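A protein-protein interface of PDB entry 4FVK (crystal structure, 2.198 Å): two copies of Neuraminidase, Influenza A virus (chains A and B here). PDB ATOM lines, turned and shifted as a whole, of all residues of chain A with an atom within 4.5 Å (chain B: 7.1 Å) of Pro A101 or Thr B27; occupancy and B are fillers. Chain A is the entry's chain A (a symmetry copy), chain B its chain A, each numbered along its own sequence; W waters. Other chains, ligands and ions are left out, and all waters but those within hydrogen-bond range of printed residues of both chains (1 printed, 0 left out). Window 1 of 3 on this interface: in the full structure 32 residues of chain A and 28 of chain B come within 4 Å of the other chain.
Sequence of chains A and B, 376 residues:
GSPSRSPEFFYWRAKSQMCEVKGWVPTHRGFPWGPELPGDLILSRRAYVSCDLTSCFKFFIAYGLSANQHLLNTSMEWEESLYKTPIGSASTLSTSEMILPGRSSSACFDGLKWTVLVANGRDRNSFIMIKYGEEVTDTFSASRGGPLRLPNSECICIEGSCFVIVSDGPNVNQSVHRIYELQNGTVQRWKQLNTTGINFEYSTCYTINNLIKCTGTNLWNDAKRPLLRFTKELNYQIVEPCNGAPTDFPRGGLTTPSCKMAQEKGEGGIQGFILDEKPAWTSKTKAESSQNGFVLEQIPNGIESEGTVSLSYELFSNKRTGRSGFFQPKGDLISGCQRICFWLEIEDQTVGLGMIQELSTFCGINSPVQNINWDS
SD of Met A129 sits close to O of Pro B26.
O of Val B25 is in hydrogen-bond range of N of Cys B363 (2.8 Å). The side-chain hydroxyl (OG1) of Thr B361 sits at hydrogen-bond distance from the side-chain hydroxyl (OG1) of Thr B27, at 2.6 Å. The backbone carbonyl oxygen (O) of His B28 lies within hydrogen-bond range of the backbone NH (N) of Thr B361 (2.8 Å). The backbone carbonyl oxygen (O) of Pro A101 lies within hydrogen-bond range of the side-chain amide nitrogen (ND2) of Asn A120 (3.1 Å). N of Gly A102 lies within hydrogen-bond range of OD1 of Asn A120 (3.1 Å). The side-chain sulfur (SG) of Cys B363 is disulfide-bonded to the side-chain sulfur (SG) of Cys B341 (2.0 Å).
O of Thr B27 touches O of Ile A99, at 3.7 Å. NE2 of His B28 touches O of Ile A99, 3.9 Å away. Thr B27 touches Leu A100. Pro B26 touches Pro A101. Pro A101 touches Thr B27 (CD to O, 3.7 Å). Pro A101 touches Arg B29 (CB to CD, 3.8 Å). Asn A120 touches Trp B374. Met A129 touches Val B25 (SD to CB, 3.8 Å). Val A136 touches Thr B27 (CG2 to CG2, 3.8 Å). Val A136 touches Arg B339 (N to NH1, 3.8 Å).
Pro A101 touches three residues of chain B. Of the printed residues of chain B, Asn A120 touches Trp B374. Of the printed residues of chain B, Met A129 touches Val B25 and Pro B26. Of the printed residues of chain B, Val A136 touches Thr B27 and Arg B339. Of the printed residues of chain A, Thr B27 touches Ile A99, Leu A100, Pro A101 and Val A136. Ile B87 touches none of the printed residues of chain A. Printed residues of chain A within 4 Å of Arg B339: Val A136 (3.8 Å). Cys B363 touches none of the printed residues of chain A. The nearest printed residue of chain A that does not touch Thr B27 is Met A129 (5.5 Å).
Of the 10 printed residues of chain A, 6 touch a printed residue of chain B. Printed residues of chain A that touch a printed residue of chain B: Ile A99, Leu A100, Pro A101, Asn A120, Met A129 and Val A136. Of the 16 printed residues of chain B, 7 touch a printed residue of chain A. Hydrophobic or aromatic side chains of chain B that line the printed part of chain A: Val B25, His B28 and Trp B374. Along chain B the printed residues that touch a printed residue of chain A span positions 25 to 374. Among the printed residues, 11 pairs touch across the chains.
No position is printed for both chains. Of the 11 pairs that touch across the chains among the printed residues, none has its exchanged pair printed and touching as well.
Water W1 bridges the side-chain hydroxyl of Ser A81 and the backbone NH of Arg B29.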
ATOM      1  N   GLU A  80      14.120   7.020  -9.216  1.00  0.00           N
ATOM      2  CA  GLU A  80      13.347   7.623 -10.277  1.00  0.00           C
ATOM      3  C   GLU A  80      12.835   8.978  -9.847  1.00  0.00           C
ATOM      4  O   GLU A  80      12.245   9.130  -8.779  1.00  0.00           O
ATOM      5  CB  GLU A  80      12.163   6.728 -10.659  1.00  0.00           C
ATOM      6  CG  GLU A  80      12.535   5.294 -11.047  1.00  0.00           C
ATOM      7  CD  GLU A  80      12.218   4.280  -9.949  1.00  0.00           C
ATOM      8  OE1 GLU A  80      11.948   3.111 -10.299  1.00  0.00           O
ATOM      9  OE2 GLU A  80      12.235   4.644  -8.741  1.00  0.00           O
ATOM     10  N   SER A  81      13.024   9.963 -10.707  1.00  0.00           N
ATOM     11  CA  SER A  81      12.506  11.281 -10.438  1.00  0.00           C
ATOM     12  C   SER A  81      11.898  11.846 -11.699  1.00  0.00           C
ATOM     13  O   SER A  81      12.329  11.540 -12.794  1.00  0.00           O
ATOM     14  CB  SER A  81      13.627  12.196  -9.939  1.00  0.00           C
ATOM     15  OG  SER A  81      14.008  11.822  -8.634  1.00  0.00           O
ATOM     16  N   ILE A  99      11.623  17.907 -10.537  1.00  0.00           N
ATOM     17  CA  ILE A  99      10.378  18.365  -9.939  1.00  0.00           C
ATOM     18  C   ILE A  99      10.067  17.604  -8.650  1.00  0.00           C
ATOM     19  O   ILE A  99       9.845  18.218  -7.614  1.00  0.00           O
ATOM     20  CB  ILE A  99       9.157  18.154 -10.883  1.00  0.00           C
ATOM     21  CG1 ILE A  99       9.332  18.839 -12.257  1.00  0.00           C
ATOM     22  CG2 ILE A  99       7.880  18.591 -10.187  1.00  0.00           C
ATOM     23  CD1 ILE A  99       9.401  20.355 -12.210  1.00  0.00           C
ATOM     24  N   LEU A 100      10.032  16.268  -8.744  1.00  0.00           N
ATOM     25  CA  LEU A 100       9.697  15.376  -7.631  1.00  0.00           C
ATOM     26  C   LEU A 100      10.212  13.965  -7.917  1.00  0.00           C
ATOM     27  O   LEU A 100      10.406  13.584  -9.076  1.00  0.00           O
ATOM     28  CB  LEU A 100       8.171  15.307  -7.392  1.00  0.00           C
ATOM     29  CG  LEU A 100       7.429  16.307  -6.482  1.00  0.00           C
ATOM     30  CD1 LEU A 100       5.933  16.116  -6.620  1.00  0.00           C
ATOM     31  CD2 LEU A 100       7.825  16.283  -4.996  1.00  0.00           C
ATOM     32  N   PRO A 101      10.437  13.178  -6.859  1.00  0.00           N
ATOM     33  CA  PRO A 101      10.720  11.751  -7.029  1.00  0.00           C
ATOM     34  C   PRO A 101       9.435  11.077  -7.549  1.00  0.00           C
ATOM     35  O   PRO A 101       8.361  11.537  -7.176  1.00  0.00           O
ATOM     36  CB  PRO A 101      11.001  11.277  -5.598  1.00  0.00           C
ATOM     37  CG  PRO A 101      11.104  12.521  -4.770  1.00  0.00           C
ATOM     38  CD  PRO A 101      10.287  13.546  -5.445  1.00  0.00           C
ATOM     39  N   GLY A 102       9.532  10.056  -8.398  1.00  0.00           N
ATOM     40  CA  GLY A 102       8.339   9.396  -8.917  1.00  0.00           C
ATOM     41  C   GLY A 102       8.665   8.388 -10.003  1.00  0.00           C
ATOM     42  O   GLY A 102       9.685   8.531 -10.668  1.00  0.00           O
ATOM     43  N   VAL A 118       2.782  12.374  -8.505  1.00  0.00           N
ATOM     44  CA  VAL A 118       3.741  11.308  -8.755  1.00  0.00           C
ATOM     45  C   VAL A 118       3.373  10.135  -7.859  1.00  0.00           C
ATOM     46  O   VAL A 118       2.764  10.317  -6.816  1.00  0.00           O
ATOM     47  CB  VAL A 118       5.206  11.716  -8.436  1.00  0.00           C
ATOM     48  CG1 VAL A 118       5.747  12.774  -9.443  1.00  0.00           C
ATOM     49  CG2 VAL A 118       5.321  12.221  -6.981  1.00  0.00           C
ATOM     50  N   ASN A 120       5.095   6.682  -5.924  1.00  0.00           N
ATOM     51  CA  ASN A 120       6.336   6.044  -5.507  1.00  0.00           C
ATOM     52  C   ASN A 120       6.060   4.799  -4.664  1.00  0.00           C
ATOM     53  O   ASN A 120       5.039   4.722  -3.977  1.00  0.00           O
ATOM     54  CB  ASN A 120       7.190   7.018  -4.687  1.00  0.00           C
ATOM     55  CG  ASN A 120       7.718   8.178  -5.510  1.00  0.00           C
ATOM     56  OD1 ASN A 120       8.781   8.082  -6.122  1.00  0.00           O
ATOM     57  ND2 ASN A 120       6.991   9.290  -5.510  1.00  0.00           N
ATOM     58  N   MET A 129       1.855  11.537  -4.182  1.00  0.00           N
ATOM     59  CA  MET A 129       2.069  12.881  -3.671  1.00  0.00           C
ATOM     60  C   MET A 129       1.573  13.918  -4.669  1.00  0.00           C
ATOM     61  O   MET A 129       1.762  13.763  -5.872  1.00  0.00           O
ATOM     62  CB  MET A 129       3.567  13.130  -3.554  1.00  0.00           C
ATOM     63  CG  MET A 129       4.167  12.940  -2.230  1.00  0.00           C
ATOM     64  SD  MET A 129       5.862  13.495  -2.414  1.00  0.00           S
ATOM     65  CE  MET A 129       6.571  12.192  -3.413  1.00  0.00           C
ATOM     66  N   VAL A 136       3.957  21.029  -1.804  1.00  0.00           N
ATOM     67  CA  VAL A 136       3.306  19.729  -1.650  1.00  0.00           C
ATOM     68  C   VAL A 136       2.013  19.908  -0.843  1.00  0.00           C
ATOM     69  O   VAL A 136       2.038  20.417   0.279  1.00  0.00           O
ATOM     70  CB  VAL A 136       4.226  18.730  -0.925  1.00  0.00           C
ATOM     71  CG1 VAL A 136       3.428  17.540  -0.419  1.00  0.00           C
ATOM     72  CG2 VAL A 136       5.365  18.277  -1.858  1.00  0.00           C
ATOM     73  N   VAL B  25       7.788  13.255   3.513  1.00  0.00           N
ATOM     74  CA  VAL B  25       7.946  12.803   2.138  1.00  0.00           C
ATOM     75  C   VAL B  25       9.076  13.577   1.471  1.00  0.00           C
ATOM     76  O   VAL B  25       9.260  14.756   1.735  1.00  0.00           O
ATOM     77  CB  VAL B  25       6.645  12.991   1.321  1.00  0.00           C
ATOM     78  CG1 VAL B  25       5.557  12.052   1.822  1.00  0.00           C
ATOM     79  CG2 VAL B  25       6.184  14.450   1.383  1.00  0.00           C
ATOM     80  N   PRO B  26       9.832  12.908   0.596  1.00  0.00           N
ATOM     81  CA  PRO B  26      10.919  13.582  -0.103  1.00  0.00           C
ATOM     82  C   PRO B  26      10.343  14.434  -1.208  1.00  0.00           C
ATOM     83  O   PRO B  26       9.499  13.967  -1.992  1.00  0.00           O
ATOM     84  CB  PRO B  26      11.746  12.429  -0.668  1.00  0.00           C
ATOM     85  CG  PRO B  26      10.813  11.290  -0.782  1.00  0.00           C
ATOM     86  CD  PRO B  26       9.733  11.481   0.243  1.00  0.00           C
ATOM     87  N   THR B  27      10.745  15.696  -1.218  1.00  0.00           N
ATOM     88  CA  THR B  27      10.377  16.597  -2.280  1.00  0.00           C
ATOM     89  C   THR B  27      11.484  16.624  -3.318  1.00  0.00           C
ATOM     90  O   THR B  27      11.252  16.983  -4.472  1.00  0.00           O
ATOM     91  CB  THR B  27      10.088  18.001  -1.750  1.00  0.00           C
ATOM     92  OG1 THR B  27      11.277  18.541  -1.150  1.00  0.00           O
ATOM     93  CG2 THR B  27       8.981  17.932  -0.711  1.00  0.00           C
ATOM     94  N   HIS B  28      12.680  16.216  -2.913  1.00  0.00           N
ATOM     95  CA  HIS B  28      13.784  16.051  -3.859  1.00  0.00           C
ATOM     96  C   HIS B  28      14.700  14.983  -3.340  1.00  0.00           C
ATOM     97  O   HIS B  28      15.202  15.094  -2.218  1.00  0.00           O
ATOM     98  CB  HIS B  28      14.614  17.346  -4.009  1.00  0.00           C
ATOM     99  CG  HIS B  28      13.855  18.491  -4.599  1.00  0.00           C
ATOM    100  ND1 HIS B  28      13.196  19.423  -3.829  1.00  0.00           N
ATOM    101  CD2 HIS B  28      13.660  18.861  -5.887  1.00  0.00           C
ATOM    102  CE1 HIS B  28      12.613  20.310  -4.616  1.00  0.00           C
ATOM    103  NE2 HIS B  28      12.883  19.993  -5.872  1.00  0.00           N
ATOM    104  N   ARG B  29      14.962  13.962  -4.142  1.00  0.00           N
ATOM    105  CA  ARG B  29      16.058  13.060  -3.821  1.00  0.00           C
ATOM    106  C   ARG B  29      17.320  13.784  -4.254  1.00  0.00           C
ATOM    107  O   ARG B  29      17.245  14.777  -4.990  1.00  0.00           O
ATOM    108  CB  ARG B  29      15.886  11.721  -4.537  1.00  0.00           C
ATOM    109  CG  ARG B  29      14.606  10.995  -4.087  1.00  0.00           C
ATOM    110  CD  ARG B  29      14.401   9.663  -4.795  1.00  0.00           C
ATOM    111  NE  ARG B  29      15.073   8.565  -4.105  1.00  0.00           N
ATOM    112  CZ  ARG B  29      14.744   7.290  -4.243  1.00  0.00           C
ATOM    113  NH1 ARG B  29      13.738   6.949  -5.034  1.00  0.00           N
ATOM    114  NH2 ARG B  29      15.414   6.357  -3.580  1.00  0.00           N
ATOM    115  N   ILE B  87      17.093  24.408  -6.398  1.00  0.00           N
ATOM    116  CA  ILE B  87      17.030  23.018  -5.881  1.00  0.00           C
ATOM    117  C   ILE B  87      16.873  22.020  -6.999  1.00  0.00           C
ATOM    118  O   ILE B  87      17.435  20.938  -6.937  1.00  0.00           O
ATOM    119  CB  ILE B  87      15.820  22.681  -4.947  1.00  0.00           C
ATOM    120  CG1 ILE B  87      14.792  23.797  -4.914  1.00  0.00           C
ATOM    121  CG2 ILE B  87      16.279  22.173  -3.582  1.00  0.00           C
ATOM    122  CD1 ILE B  87      13.712  23.587  -5.899  1.00  0.00           C
ATOM    123  N   PHE B 327      14.729  23.564   6.910  1.00  0.00           N
ATOM    124  CA  PHE B 327      14.444  24.786   6.157  1.00  0.00           C
ATOM    125  C   PHE B 327      12.938  25.001   6.140  1.00  0.00           C
ATOM    126  O   PHE B 327      12.187  24.062   6.315  1.00  0.00           O
ATOM    127  CB  PHE B 327      15.070  24.774   4.753  1.00  0.00           C
ATOM    128  CG  PHE B 327      14.388  23.834   3.771  1.00  0.00           C
ATOM    129  CD1 PHE B 327      14.752  22.495   3.703  1.00  0.00           C
ATOM    130  CD2 PHE B 327      13.408  24.299   2.914  1.00  0.00           C
ATOM    131  CE1 PHE B 327      14.135  21.624   2.800  1.00  0.00           C
ATOM    132  CE2 PHE B 327      12.792  23.439   1.991  1.00  0.00           C
ATOM    133  CZ  PHE B 327      13.163  22.101   1.940  1.00  0.00           C
ATOM    134  N   ARG B 339       4.552  25.029   7.198  1.00  0.00           N
ATOM    135  CA  ARG B 339       5.186  23.743   6.934  1.00  0.00           C
ATOM    136  C   ARG B 339       6.627  23.747   7.426  1.00  0.00           C
ATOM    137  O   ARG B 339       7.262  24.810   7.560  1.00  0.00           O
ATOM    138  CB  ARG B 339       5.166  23.414   5.422  1.00  0.00           C
ATOM    139  CG  ARG B 339       3.790  23.033   4.881  1.00  0.00           C
ATOM    140  CD  ARG B 339       3.863  22.409   3.491  1.00  0.00           C
ATOM    141  NE  ARG B 339       4.532  23.263   2.507  1.00  0.00           N
ATOM    142  CZ  ARG B 339       5.404  22.806   1.618  1.00  0.00           C
ATOM    143  NH1 ARG B 339       5.692  21.504   1.588  1.00  0.00           N
ATOM    144  NH2 ARG B 339       5.971  23.635   0.751  1.00  0.00           N
ATOM    145  N   CYS B 341      10.364  21.569   6.761  1.00  0.00           N
ATOM    146  CA  CYS B 341      11.136  20.615   5.981  1.00  0.00           C
ATOM    147  C   CYS B 341      12.552  20.447   6.524  1.00  0.00           C
ATOM    148  O   CYS B 341      12.967  21.175   7.417  1.00  0.00           O
ATOM    149  CB  CYS B 341      11.220  21.058   4.518  1.00  0.00           C
ATOM    150  SG  CYS B 341       9.641  21.532   3.766  1.00  0.00           S
ATOM    151  N   PHE B 342      13.274  19.460   6.000  1.00  0.00           N
ATOM    152  CA  PHE B 342      14.692  19.290   6.300  1.00  0.00           C
ATOM    153  C   PHE B 342      15.496  18.887   5.074  1.00  0.00           C
ATOM    154  O   PHE B 342      14.974  18.295   4.132  1.00  0.00           O
ATOM    155  CB  PHE B 342      14.959  18.318   7.479  1.00  0.00           C
ATOM    156  CG  PHE B 342      14.596  16.855   7.230  1.00  0.00           C
ATOM    157  CD1 PHE B 342      13.368  16.351   7.645  1.00  0.00           C
ATOM    158  CD2 PHE B 342      15.521  15.970   6.696  1.00  0.00           C
ATOM    159  CE1 PHE B 342      13.019  14.983   7.451  1.00  0.00           C
ATOM    160  CE2 PHE B 342      15.204  14.622   6.497  1.00  0.00           C
ATOM    161  CZ  PHE B 342      13.938  14.117   6.889  1.00  0.00           C
ATOM    162  N   SER B 360      19.268  15.762  -0.233  1.00  0.00           N
ATOM    163  CA  SER B 360      17.869  15.466  -0.457  1.00  0.00           C
ATOM    164  C   SER B 360      17.052  16.366   0.465  1.00  0.00           C
ATOM    165  O   SER B 360      17.551  16.846   1.488  1.00  0.00           O
ATOM    166  CB  SER B 360      17.560  14.001  -0.145  1.00  0.00           C
ATOM    167  OG  SER B 360      17.724  13.785   1.251  1.00  0.00           O
ATOM    168  N   THR B 361      15.805  16.617   0.092  1.00  0.00           N
ATOM    169  CA  THR B 361      14.918  17.414   0.932  1.00  0.00           C
ATOM    170  C   THR B 361      13.638  16.645   1.220  1.00  0.00           C
ATOM    171  O   THR B 361      13.083  16.003   0.326  1.00  0.00           O
ATOM    172  CB  THR B 361      14.573  18.764   0.299  1.00  0.00           C
ATOM    173  OG1 THR B 361      13.900  18.568  -0.965  1.00  0.00           O
ATOM    174  CG2 THR B 361      15.850  19.600   0.090  1.00  0.00           C
ATOM    175  N   PHE B 362      13.185  16.711   2.471  1.00  0.00           N
ATOM    176  CA  PHE B 362      11.963  16.052   2.918  1.00  0.00           C
ATOM    177  C   PHE B 362      11.072  17.091   3.585  1.00  0.00           C
ATOM    178  O   PHE B 362      11.566  17.950   4.292  1.00  0.00           O
ATOM    179  CB  PHE B 362      12.299  14.965   3.938  1.00  0.00           C
ATOM    180  CG  PHE B 362      12.889  13.714   3.342  1.00  0.00           C
ATOM    181  CD1 PHE B 362      14.227  13.662   2.958  1.00  0.00           C
ATOM    182  CD2 PHE B 362      12.108  12.585   3.175  1.00  0.00           C
ATOM    183  CE1 PHE B 362      14.766  12.499   2.413  1.00  0.00           C
ATOM    184  CE2 PHE B 362      12.635  11.415   2.635  1.00  0.00           C
ATOM    185  CZ  PHE B 362      13.955  11.365   2.259  1.00  0.00           C
ATOM    186  N   CYS B 363       9.762  17.032   3.371  1.00  0.00           N
ATOM    187  CA  CYS B 363       8.857  17.937   4.096  1.00  0.00           C
ATOM    188  C   CYS B 363       7.834  17.175   4.961  1.00  0.00           C
ATOM    189  O   CYS B 363       7.467  16.051   4.652  1.00  0.00           O
ATOM    190  CB  CYS B 363       8.150  18.910   3.137  1.00  0.00           C
ATOM    191  SG  CYS B 363       9.257  20.127   2.325  1.00  0.00           S
ATOM    192  N   GLY B 364       7.387  17.790   6.046  1.00  0.00           N
ATOM    193  CA  GLY B 364       6.391  17.173   6.903  1.00  0.00           C
ATOM    194  C   GLY B 364       5.016  17.218   6.255  1.00  0.00           C
ATOM    195  O   GLY B 364       4.678  18.186   5.581  1.00  0.00           O
ATOM    196  N   TRP B 374      13.893   4.654   1.250  1.00  0.00           N
ATOM    197  CA  TRP B 374      14.300   5.470   0.084  1.00  0.00           C
ATOM    198  C   TRP B 374      15.686   5.156  -0.486  1.00  0.00           C
ATOM    199  O   TRP B 374      16.148   5.871  -1.365  1.00  0.00           O
ATOM    200  CB  TRP B 374      14.153   6.986   0.336  1.00  0.00           C
ATOM    201  CG  TRP B 374      12.743   7.383   0.584  1.00  0.00           C
ATOM    202  CD1 TRP B 374      12.152   7.571   1.802  1.00  0.00           C
ATOM    203  CD2 TRP B 374      11.720   7.591  -0.392  1.00  0.00           C
ATOM    204  NE1 TRP B 374      10.834   7.885   1.649  1.00  0.00           N
ATOM    205  CE2 TRP B 374      10.535   7.907   0.311  1.00  0.00           C
ATOM    206  CE3 TRP B 374      11.691   7.557  -1.796  1.00  0.00           C
ATOM    207  CZ2 TRP B 374       9.334   8.178  -0.330  1.00  0.00           C
ATOM    208  CZ3 TRP B 374      10.489   7.835  -2.438  1.00  0.00           C
ATOM    209  CH2 TRP B 374       9.330   8.148  -1.702  1.00  0.00           C
HETATM  210  O   HOH W   1      13.653  13.942  -6.892  1.00  0.00           O
